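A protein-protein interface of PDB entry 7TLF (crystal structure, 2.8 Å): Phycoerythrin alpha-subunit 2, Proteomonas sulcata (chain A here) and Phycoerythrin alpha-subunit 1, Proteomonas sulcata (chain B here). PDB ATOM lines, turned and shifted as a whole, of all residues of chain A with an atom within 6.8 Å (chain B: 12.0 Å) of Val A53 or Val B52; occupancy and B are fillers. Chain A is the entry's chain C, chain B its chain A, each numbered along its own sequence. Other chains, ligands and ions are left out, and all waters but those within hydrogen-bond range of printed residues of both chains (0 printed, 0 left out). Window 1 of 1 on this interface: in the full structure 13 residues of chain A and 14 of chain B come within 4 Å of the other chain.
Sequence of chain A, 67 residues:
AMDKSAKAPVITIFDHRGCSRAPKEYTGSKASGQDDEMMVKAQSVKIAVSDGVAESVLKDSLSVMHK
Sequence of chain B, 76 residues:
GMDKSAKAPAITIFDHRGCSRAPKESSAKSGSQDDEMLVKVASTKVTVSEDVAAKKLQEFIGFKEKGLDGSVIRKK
Of chain B, only Val B52 comes within 4 Å of Val A53. Of the printed residues of chain A, Val B52 touches Ser A50 and Val A53. No residue of chain B comes within 4 Å of Val A49. No residue of chain B comes within 4 Å of Gly A52. No residue of chain B comes within 4 Å of Ala A54. No residue of chain B comes within 4 Å of Glu A55. Of the printed residues of chain A, Ser B49 touches Ser A50 (3.3 Å). Thr B47 touches none of the printed residues of chain A. Lys B55 touches none of the printed residues of chain A. The nearest residue of chain B that does not touch Val A53 is Ser B49 (5.4 Å). The nearest residue of chain A that does not touch Val B52 is Gly A52 (6.5 Å).
Among the printed residues, pairs that only touch across the chains: Ser A50 with Val B52 (3.7 Å) and Val A53 with Val B52 (3.4 Å).
The side-chain hydroxyl (OG) of Ser B49 lies within hydrogen-bond range of the side-chain hydroxyl (OG) of Ser A50 (3.3 Å).
Hydrophobic or aromatic side chains of chain A that line the printed part of chain B: Val A53. Among the printed residues, 3 pairs touch across the chains.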
ATOM      1  N   VAL A  49      14.016  -8.087  16.671  1.00  0.00           N
ATOM      2  CA  VAL A  49      12.787  -8.391  17.396  1.00  0.00           C
ATOM      3  C   VAL A  49      11.758  -7.307  17.111  1.00  0.00           C
ATOM      4  O   VAL A  49      12.055  -6.113  17.229  1.00  0.00           O
ATOM      5  CB  VAL A  49      13.042  -8.501  18.914  1.00  0.00           C
ATOM      6  CG1 VAL A  49      11.739  -8.744  19.664  1.00  0.00           C
ATOM      7  CG2 VAL A  49      14.042  -9.608  19.199  1.00  0.00           C
ATOM      8  N   SER A  50      10.557  -7.723  16.713  1.00  0.00           N
ATOM      9  CA  SER A  50       9.525  -6.766  16.358  1.00  0.00           C
ATOM     10  C   SER A  50       8.895  -6.170  17.614  1.00  0.00           C
ATOM     11  O   SER A  50       9.018  -6.702  18.720  1.00  0.00           O
ATOM     12  CB  SER A  50       8.447  -7.420  15.490  1.00  0.00           C
ATOM     13  OG  SER A  50       7.901  -8.568  16.117  1.00  0.00           O
ATOM     14  N   ASP A  51       8.188  -5.060  17.423  1.00  0.00           N
ATOM     15  CA  ASP A  51       7.497  -4.435  18.543  1.00  0.00           C
ATOM     16  C   ASP A  51       6.380  -5.318  19.078  1.00  0.00           C
ATOM     17  O   ASP A  51       6.045  -5.235  20.263  1.00  0.00           O
ATOM     18  CB  ASP A  51       6.957  -3.065  18.142  1.00  0.00           C
ATOM     19  CG  ASP A  51       8.054  -2.029  18.017  1.00  0.00           C
ATOM     20  OD1 ASP A  51       8.931  -1.984  18.906  1.00  0.00           O
ATOM     21  OD2 ASP A  51       8.037  -1.258  17.037  1.00  0.00           O
ATOM     22  N   GLY A  52       5.803  -6.179  18.237  1.00  0.00           N
ATOM     23  CA  GLY A  52       4.729  -7.031  18.717  1.00  0.00           C
ATOM     24  C   GLY A  52       5.207  -8.091  19.687  1.00  0.00           C
ATOM     25  O   GLY A  52       4.535  -8.373  20.683  1.00  0.00           O
ATOM     26  N   VAL A  53       6.362  -8.709  19.413  1.00  0.00           N
ATOM     27  CA  VAL A  53       6.891  -9.660  20.387  1.00  0.00           C
ATOM     28  C   VAL A  53       7.205  -8.936  21.687  1.00  0.00           C
ATOM     29  O   VAL A  53       7.003  -9.478  22.780  1.00  0.00           O
ATOM     30  CB  VAL A  53       8.119 -10.409  19.835  1.00  0.00           C
ATOM     31  CG1 VAL A  53       8.639 -11.400  20.858  1.00  0.00           C
ATOM     32  CG2 VAL A  53       7.739 -11.155  18.592  1.00  0.00           C
ATOM     33  N   ALA A  54       7.777  -7.730  21.591  1.00  0.00           N
ATOM     34  CA  ALA A  54       8.070  -6.981  22.805  1.00  0.00           C
ATOM     35  C   ALA A  54       6.795  -6.703  23.596  1.00  0.00           C
ATOM     36  O   ALA A  54       6.783  -6.810  24.829  1.00  0.00           O
ATOM     37  CB  ALA A  54       8.784  -5.679  22.451  1.00  0.00           C
ATOM     38  N   GLU A  55       5.694  -6.384  22.899  1.00  0.00           N
ATOM     39  CA  GLU A  55       4.448  -6.100  23.602  1.00  0.00           C
ATOM     40  C   GLU A  55       3.856  -7.364  24.196  1.00  0.00           C
ATOM     41  O   GLU A  55       3.247  -7.317  25.266  1.00  0.00           O
ATOM     42  CB  GLU A  55       3.425  -5.429  22.685  1.00  0.00           C
ATOM     43  CG  GLU A  55       3.859  -4.105  22.089  1.00  0.00           C
ATOM     44  CD  GLU A  55       2.745  -3.426  21.302  1.00  0.00           C
ATOM     45  OE1 GLU A  55       2.109  -4.102  20.465  1.00  0.00           O
ATOM     46  OE2 GLU A  55       2.509  -2.217  21.512  1.00  0.00           O
ATOM     47  N   SER A  56       4.082  -8.507  23.551  1.00  0.00           N
ATOM     48  CA  SER A  56       3.581  -9.757  24.103  1.00  0.00           C
ATOM     49  C   SER A  56       4.372 -10.162  25.334  1.00  0.00           C
ATOM     50  O   SER A  56       3.793 -10.588  26.339  1.00  0.00           O
ATOM     51  CB  SER A  56       3.628 -10.860  23.052  1.00  0.00           C
ATOM     52  OG  SER A  56       3.128 -12.073  23.587  1.00  0.00           O
ATOM     53  N   VAL A  57       5.698 -10.056  25.264  1.00  0.00           N
ATOM     54  CA  VAL A  57       6.537 -10.333  26.425  1.00  0.00           C
ATOM     55  C   VAL A  57       6.208  -9.379  27.566  1.00  0.00           C
ATOM     56  O   VAL A  57       6.200  -9.772  28.737  1.00  0.00           O
ATOM     57  CB  VAL A  57       8.025 -10.279  26.036  1.00  0.00           C
ATOM     58  CG1 VAL A  57       8.912 -10.349  27.285  1.00  0.00           C
ATOM     59  CG2 VAL A  57       8.342 -11.400  25.062  1.00  0.00           C
ATOM     60  N   LEU A  58       5.887  -8.125  27.247  1.00  0.00           N
ATOM     61  CA  LEU A  58       5.475  -7.179  28.281  1.00  0.00           C
ATOM     62  C   LEU A  58       4.147  -7.600  28.910  1.00  0.00           C
ATOM     63  O   LEU A  58       4.015  -7.651  30.140  1.00  0.00           O
ATOM     64  CB  LEU A  58       5.406  -5.772  27.691  1.00  0.00           C
ATOM     65  CG  LEU A  58       4.799  -4.685  28.571  1.00  0.00           C
ATOM     66  CD1 LEU A  58       5.543  -4.592  29.891  1.00  0.00           C
ATOM     67  CD2 LEU A  58       4.867  -3.363  27.834  1.00  0.00           C
ATOM     68  N   LYS A  59       3.141  -7.872  28.077  1.00  0.00           N
ATOM     69  CA  LYS A  59       1.833  -8.279  28.571  1.00  0.00           C
ATOM     70  C   LYS A  59       1.945  -9.542  29.418  1.00  0.00           C
ATOM     71  O   LYS A  59       1.249  -9.684  30.431  1.00  0.00           O
ATOM     72  CB  LYS A  59       0.892  -8.500  27.383  1.00  0.00           C
ATOM     73  CG  LYS A  59      -0.588  -8.218  27.627  1.00  0.00           C
ATOM     74  CD  LYS A  59      -1.306  -9.394  28.278  1.00  0.00           C
ATOM     75  CE  LYS A  59      -1.959 -10.312  27.251  1.00  0.00           C
ATOM     76  NZ  LYS A  59      -0.965 -11.002  26.372  1.00  0.00           N
ATOM     77  N   THR B  44      -8.357  -6.295  20.392  1.00  0.00           N
ATOM     78  CA  THR B  44      -7.214  -5.843  19.614  1.00  0.00           C
ATOM     79  C   THR B  44      -7.078  -6.714  18.377  1.00  0.00           C
ATOM     80  O   THR B  44      -7.425  -7.897  18.396  1.00  0.00           O
ATOM     81  CB  THR B  44      -5.907  -5.918  20.433  1.00  0.00           C
ATOM     82  OG1 THR B  44      -6.127  -5.430  21.765  1.00  0.00           O
ATOM     83  CG2 THR B  44      -4.799  -5.109  19.768  1.00  0.00           C
ATOM     84  N   LYS B  45      -6.613  -6.113  17.284  1.00  0.00           N
ATOM     85  CA  LYS B  45      -6.329  -6.894  16.090  1.00  0.00           C
ATOM     86  C   LYS B  45      -5.077  -7.731  16.314  1.00  0.00           C
ATOM     87  O   LYS B  45      -4.006  -7.190  16.608  1.00  0.00           O
ATOM     88  CB  LYS B  45      -6.172  -5.994  14.867  1.00  0.00           C
ATOM     89  CG  LYS B  45      -6.035  -6.779  13.564  1.00  0.00           C
ATOM     90  CD  LYS B  45      -6.010  -5.871  12.346  1.00  0.00           C
ATOM     91  CE  LYS B  45      -6.076  -6.685  11.062  1.00  0.00           C
ATOM     92  NZ  LYS B  45      -6.005  -5.829   9.846  1.00  0.00           N
ATOM     93  N   VAL B  46      -5.205  -9.040  16.166  1.00  0.00           N
ATOM     94  CA  VAL B  46      -4.062  -9.931  16.310  1.00  0.00           C
ATOM     95  C   VAL B  46      -3.288  -9.931  15.003  1.00  0.00           C
ATOM     96  O   VAL B  46      -3.865 -10.123  13.928  1.00  0.00           O
ATOM     97  CB  VAL B  46      -4.523 -11.344  16.688  1.00  0.00           C
ATOM     98  CG1 VAL B  46      -3.337 -12.242  16.880  1.00  0.00           C
ATOM     99  CG2 VAL B  46      -5.341 -11.291  17.962  1.00  0.00           C
ATOM    100  N   THR B  47      -1.988  -9.670  15.082  1.00  0.00           N
ATOM    101  CA  THR B  47      -1.139  -9.704  13.900  1.00  0.00           C
ATOM    102  C   THR B  47       0.167 -10.396  14.249  1.00  0.00           C
ATOM    103  O   THR B  47       0.713 -10.194  15.335  1.00  0.00           O
ATOM    104  CB  THR B  47      -0.854  -8.301  13.349  1.00  0.00           C
ATOM    105  OG1 THR B  47      -0.304  -7.479  14.385  1.00  0.00           O
ATOM    106  CG2 THR B  47      -2.129  -7.659  12.797  1.00  0.00           C
ATOM    107  N   VAL B  48       0.653 -11.222  13.328  1.00  0.00           N
ATOM    108  CA  VAL B  48       1.936 -11.899  13.463  1.00  0.00           C
ATOM    109  C   VAL B  48       2.845 -11.412  12.346  1.00  0.00           C
ATOM    110  O   VAL B  48       2.513 -11.563  11.166  1.00  0.00           O
ATOM    111  CB  VAL B  48       1.785 -13.428  13.418  1.00  0.00           C
ATOM    112  CG1 VAL B  48       3.148 -14.091  13.392  1.00  0.00           C
ATOM    113  CG2 VAL B  48       0.977 -13.909  14.613  1.00  0.00           C
ATOM    114  N   SER B  49       3.958 -10.782  12.714  1.00  0.00           N
ATOM    115  CA  SER B  49       4.850 -10.198  11.721  1.00  0.00           C
ATOM    116  C   SER B  49       5.514 -11.312  10.921  1.00  0.00           C
ATOM    117  O   SER B  49       5.913 -12.343  11.471  1.00  0.00           O
ATOM    118  CB  SER B  49       5.898  -9.307  12.385  1.00  0.00           C
ATOM    119  OG  SER B  49       6.466  -9.936  13.515  1.00  0.00           O
ATOM    120  N   GLU B  50       5.629 -11.101   9.609  1.00  0.00           N
ATOM    121  CA  GLU B  50       6.288 -12.075   8.748  1.00  0.00           C
ATOM    122  C   GLU B  50       7.742 -12.342   9.137  1.00  0.00           C
ATOM    123  O   GLU B  50       8.262 -13.424   8.833  1.00  0.00           O
ATOM    124  CB  GLU B  50       6.186 -11.588   7.308  1.00  0.00           C
ATOM    125  CG  GLU B  50       4.863 -11.941   6.654  1.00  0.00           C
ATOM    126  CD  GLU B  50       4.778 -11.458   5.227  1.00  0.00           C
ATOM    127  OE1 GLU B  50       4.226 -10.358   5.012  1.00  0.00           O
ATOM    128  OE2 GLU B  50       5.276 -12.165   4.326  1.00  0.00           O
ATOM    129  N   ASP B  51       8.387 -11.422   9.859  1.00  0.00           N
ATOM    130  CA  ASP B  51       9.683 -11.725  10.464  1.00  0.00           C
ATOM    131  C   ASP B  51       9.531 -12.827  11.503  1.00  0.00           C
ATOM    132  O   ASP B  51      10.319 -13.782  11.548  1.00  0.00           O
ATOM    133  CB  ASP B  51      10.279 -10.466  11.089  1.00  0.00           C
ATOM    134  CG  ASP B  51      10.419  -9.336  10.093  1.00  0.00           C
ATOM    135  OD1 ASP B  51      10.588  -9.628   8.892  1.00  0.00           O
ATOM    136  OD2 ASP B  51      10.352  -8.160  10.508  1.00  0.00           O
ATOM    137  N   VAL B  52       8.551 -12.666  12.391  1.00  0.00           N
ATOM    138  CA  VAL B  52       8.293 -13.661  13.424  1.00  0.00           C
ATOM    139  C   VAL B  52       7.985 -15.001  12.776  1.00  0.00           C
ATOM    140  O   VAL B  52       8.498 -16.040  13.197  1.00  0.00           O
ATOM    141  CB  VAL B  52       7.161 -13.194  14.351  1.00  0.00           C
ATOM    142  CG1 VAL B  52       6.554 -14.377  15.100  1.00  0.00           C
ATOM    143  CG2 VAL B  52       7.686 -12.154  15.301  1.00  0.00           C
ATOM    144  N   ALA B  53       7.051 -15.006  11.818  1.00  0.00           N
ATOM    145  CA  ALA B  53       6.722 -16.228  11.090  1.00  0.00           C
ATOM    146  C   ALA B  53       7.958 -16.876  10.467  1.00  0.00           C
ATOM    147  O   ALA B  53       8.081 -18.105  10.454  1.00  0.00           O
ATOM    148  CB  ALA B  53       5.688 -15.921  10.009  1.00  0.00           C
ATOM    149  N   ALA B  54       8.892 -16.070   9.960  1.00  0.00           N
ATOM    150  CA  ALA B  54      10.118 -16.628   9.388  1.00  0.00           C
ATOM    151  C   ALA B  54      10.980 -17.296  10.458  1.00  0.00           C
ATOM    152  O   ALA B  54      11.442 -18.435  10.285  1.00  0.00           O
ATOM    153  CB  ALA B  54      10.909 -15.540   8.662  1.00  0.00           C
ATOM    154  N   LYS B  55      11.205 -16.599  11.576  1.00  0.00           N
ATOM    155  CA  LYS B  55      11.940 -17.202  12.687  1.00  0.00           C
ATOM    156  C   LYS B  55      11.239 -18.449  13.221  1.00  0.00           C
ATOM    157  O   LYS B  55      11.900 -19.416  13.637  1.00  0.00           O
ATOM    158  CB  LYS B  55      12.112 -16.159  13.791  1.00  0.00           C
ATOM    159  CG  LYS B  55      13.059 -15.046  13.388  1.00  0.00           C
ATOM    160  CD  LYS B  55      13.163 -13.922  14.407  1.00  0.00           C
ATOM    161  CE  LYS B  55      13.977 -14.312  15.617  1.00  0.00           C
ATOM    162  NZ  LYS B  55      14.089 -13.157  16.548  1.00  0.00           N
ATOM    163  N   LYS B  56       9.910 -18.484  13.153  1.00  0.00           N
ATOM    164  CA  LYS B  56       9.212 -19.664  13.633  1.00  0.00           C
ATOM    165  C   LYS B  56       9.403 -20.805  12.649  1.00  0.00           C
ATOM    166  O   LYS B  56       9.555 -21.961  13.049  1.00  0.00           O
ATOM    167  CB  LYS B  56       7.729 -19.355  13.842  1.00  0.00           C
ATOM    168  CG  LYS B  56       7.466 -18.368  14.975  1.00  0.00           C
ATOM    169  CD  LYS B  56       8.311 -18.676  16.205  1.00  0.00           C
ATOM    170  CE  LYS B  56       7.838 -19.920  16.927  1.00  0.00           C
ATOM    171  NZ  LYS B  56       8.496 -20.042  18.254  1.00  0.00           N
ATOM    172  N   LEU B  57       9.445 -20.482  11.353  1.00  0.00           N
ATOM    173  CA  LEU B  57       9.721 -21.500  10.352  1.00  0.00           C
ATOM    174  C   LEU B  57      11.099 -22.087  10.594  1.00  0.00           C
ATOM    175  O   LEU B  57      11.323 -23.284  10.383  1.00  0.00           O
ATOM    176  CB  LEU B  57       9.632 -20.884   8.956  1.00  0.00           C
ATOM    177  CG  LEU B  57      10.064 -21.723   7.755  1.00  0.00           C
ATOM    178  CD1 LEU B  57       9.150 -22.929   7.599  1.00  0.00           C
ATOM    179  CD2 LEU B  57      10.124 -20.881   6.486  1.00  0.00           C
ATOM    180  N   GLN B  58      12.029 -21.248  11.051  1.00  0.00           N
ATOM    181  CA  GLN B  58      13.387 -21.715  11.300  1.00  0.00           C
ATOM    182  C   GLN B  58      13.437 -22.642  12.508  1.00  0.00           C
ATOM    183  O   GLN B  58      14.202 -23.613  12.522  1.00  0.00           O
ATOM    184  CB  GLN B  58      14.308 -20.512  11.504  1.00  0.00           C
ATOM    185  CG  GLN B  58      15.784 -20.832  11.584  1.00  0.00           C
ATOM    186  CD  GLN B  58      16.217 -21.206  12.991  1.00  0.00           C
ATOM    187  OE1 GLN B  58      15.474 -21.002  13.954  1.00  0.00           O
ATOM    188  NE2 GLN B  58      17.422 -21.753  13.119  1.00  0.00           N
ATOM    189  N   GLU B  59      12.612 -22.366  13.524  1.00  0.00           N
ATOM    190  CA  GLU B  59      12.509 -23.277  14.668  1.00  0.00           C
ATOM    191  C   GLU B  59      11.768 -24.573  14.329  1.00  0.00           C
ATOM    192  O   GLU B  59      12.068 -25.628  14.901  1.00  0.00           O
ATOM    193  CB  GLU B  59      11.842 -22.584  15.862  1.00  0.00           C
ATOM    194  CG  GLU B  59      12.549 -21.318  16.351  1.00  0.00           C
ATOM    195  CD  GLU B  59      11.803 -20.630  17.492  1.00  0.00           C
ATOM    196  OE1 GLU B  59      10.613 -20.942  17.697  1.00  0.00           O
ATOM    197  OE2 GLU B  59      12.396 -19.754  18.168  1.00  0.00           O
ATOM    198  N   PHE B  60      10.800 -24.514  13.410  1.00  0.00           N
ATOM    199  CA  PHE B  60       9.918 -25.646  13.127  1.00  0.00           C
ATOM    200  C   PHE B  60      10.502 -26.645  12.137  1.00  0.00           C
ATOM    201  O   PHE B  60      10.209 -27.842  12.231  1.00  0.00           O
ATOM    202  CB  PHE B  60       8.584 -25.159  12.546  1.00  0.00           C
ATOM    203  CG  PHE B  60       7.831 -24.205  13.430  1.00  0.00           C
ATOM    204  CD1 PHE B  60       8.148 -24.057  14.770  1.00  0.00           C
ATOM    205  CD2 PHE B  60       6.805 -23.438  12.903  1.00  0.00           C
ATOM    206  CE1 PHE B  60       7.457 -23.162  15.561  1.00  0.00           C
ATOM    207  CE2 PHE B  60       6.108 -22.547  13.691  1.00  0.00           C
ATOM    208  CZ  PHE B  60       6.432 -22.411  15.020  1.00  0.00           C
ATOM    209  N   ILE B  61      11.315 -26.182  11.184  1.00  0.00           N
ATOM    210  CA  ILE B  61      11.666 -26.999  10.027  1.00  0.00           C
ATOM    211  C   ILE B  61      12.555 -28.192  10.355  1.00  0.00           C
ATOM    212  O   ILE B  61      12.747 -29.055   9.490  1.00  0.00           O
ATOM    213  CB  ILE B  61      12.304 -26.106   8.947  1.00  0.00           C
ATOM    214  CG1 ILE B  61      12.153 -26.755   7.569  1.00  0.00           C
ATOM    215  CG2 ILE B  61      13.759 -25.860   9.269  1.00  0.00           C
ATOM    216  CD1 ILE B  61      12.794 -25.969   6.455  1.00  0.00           C
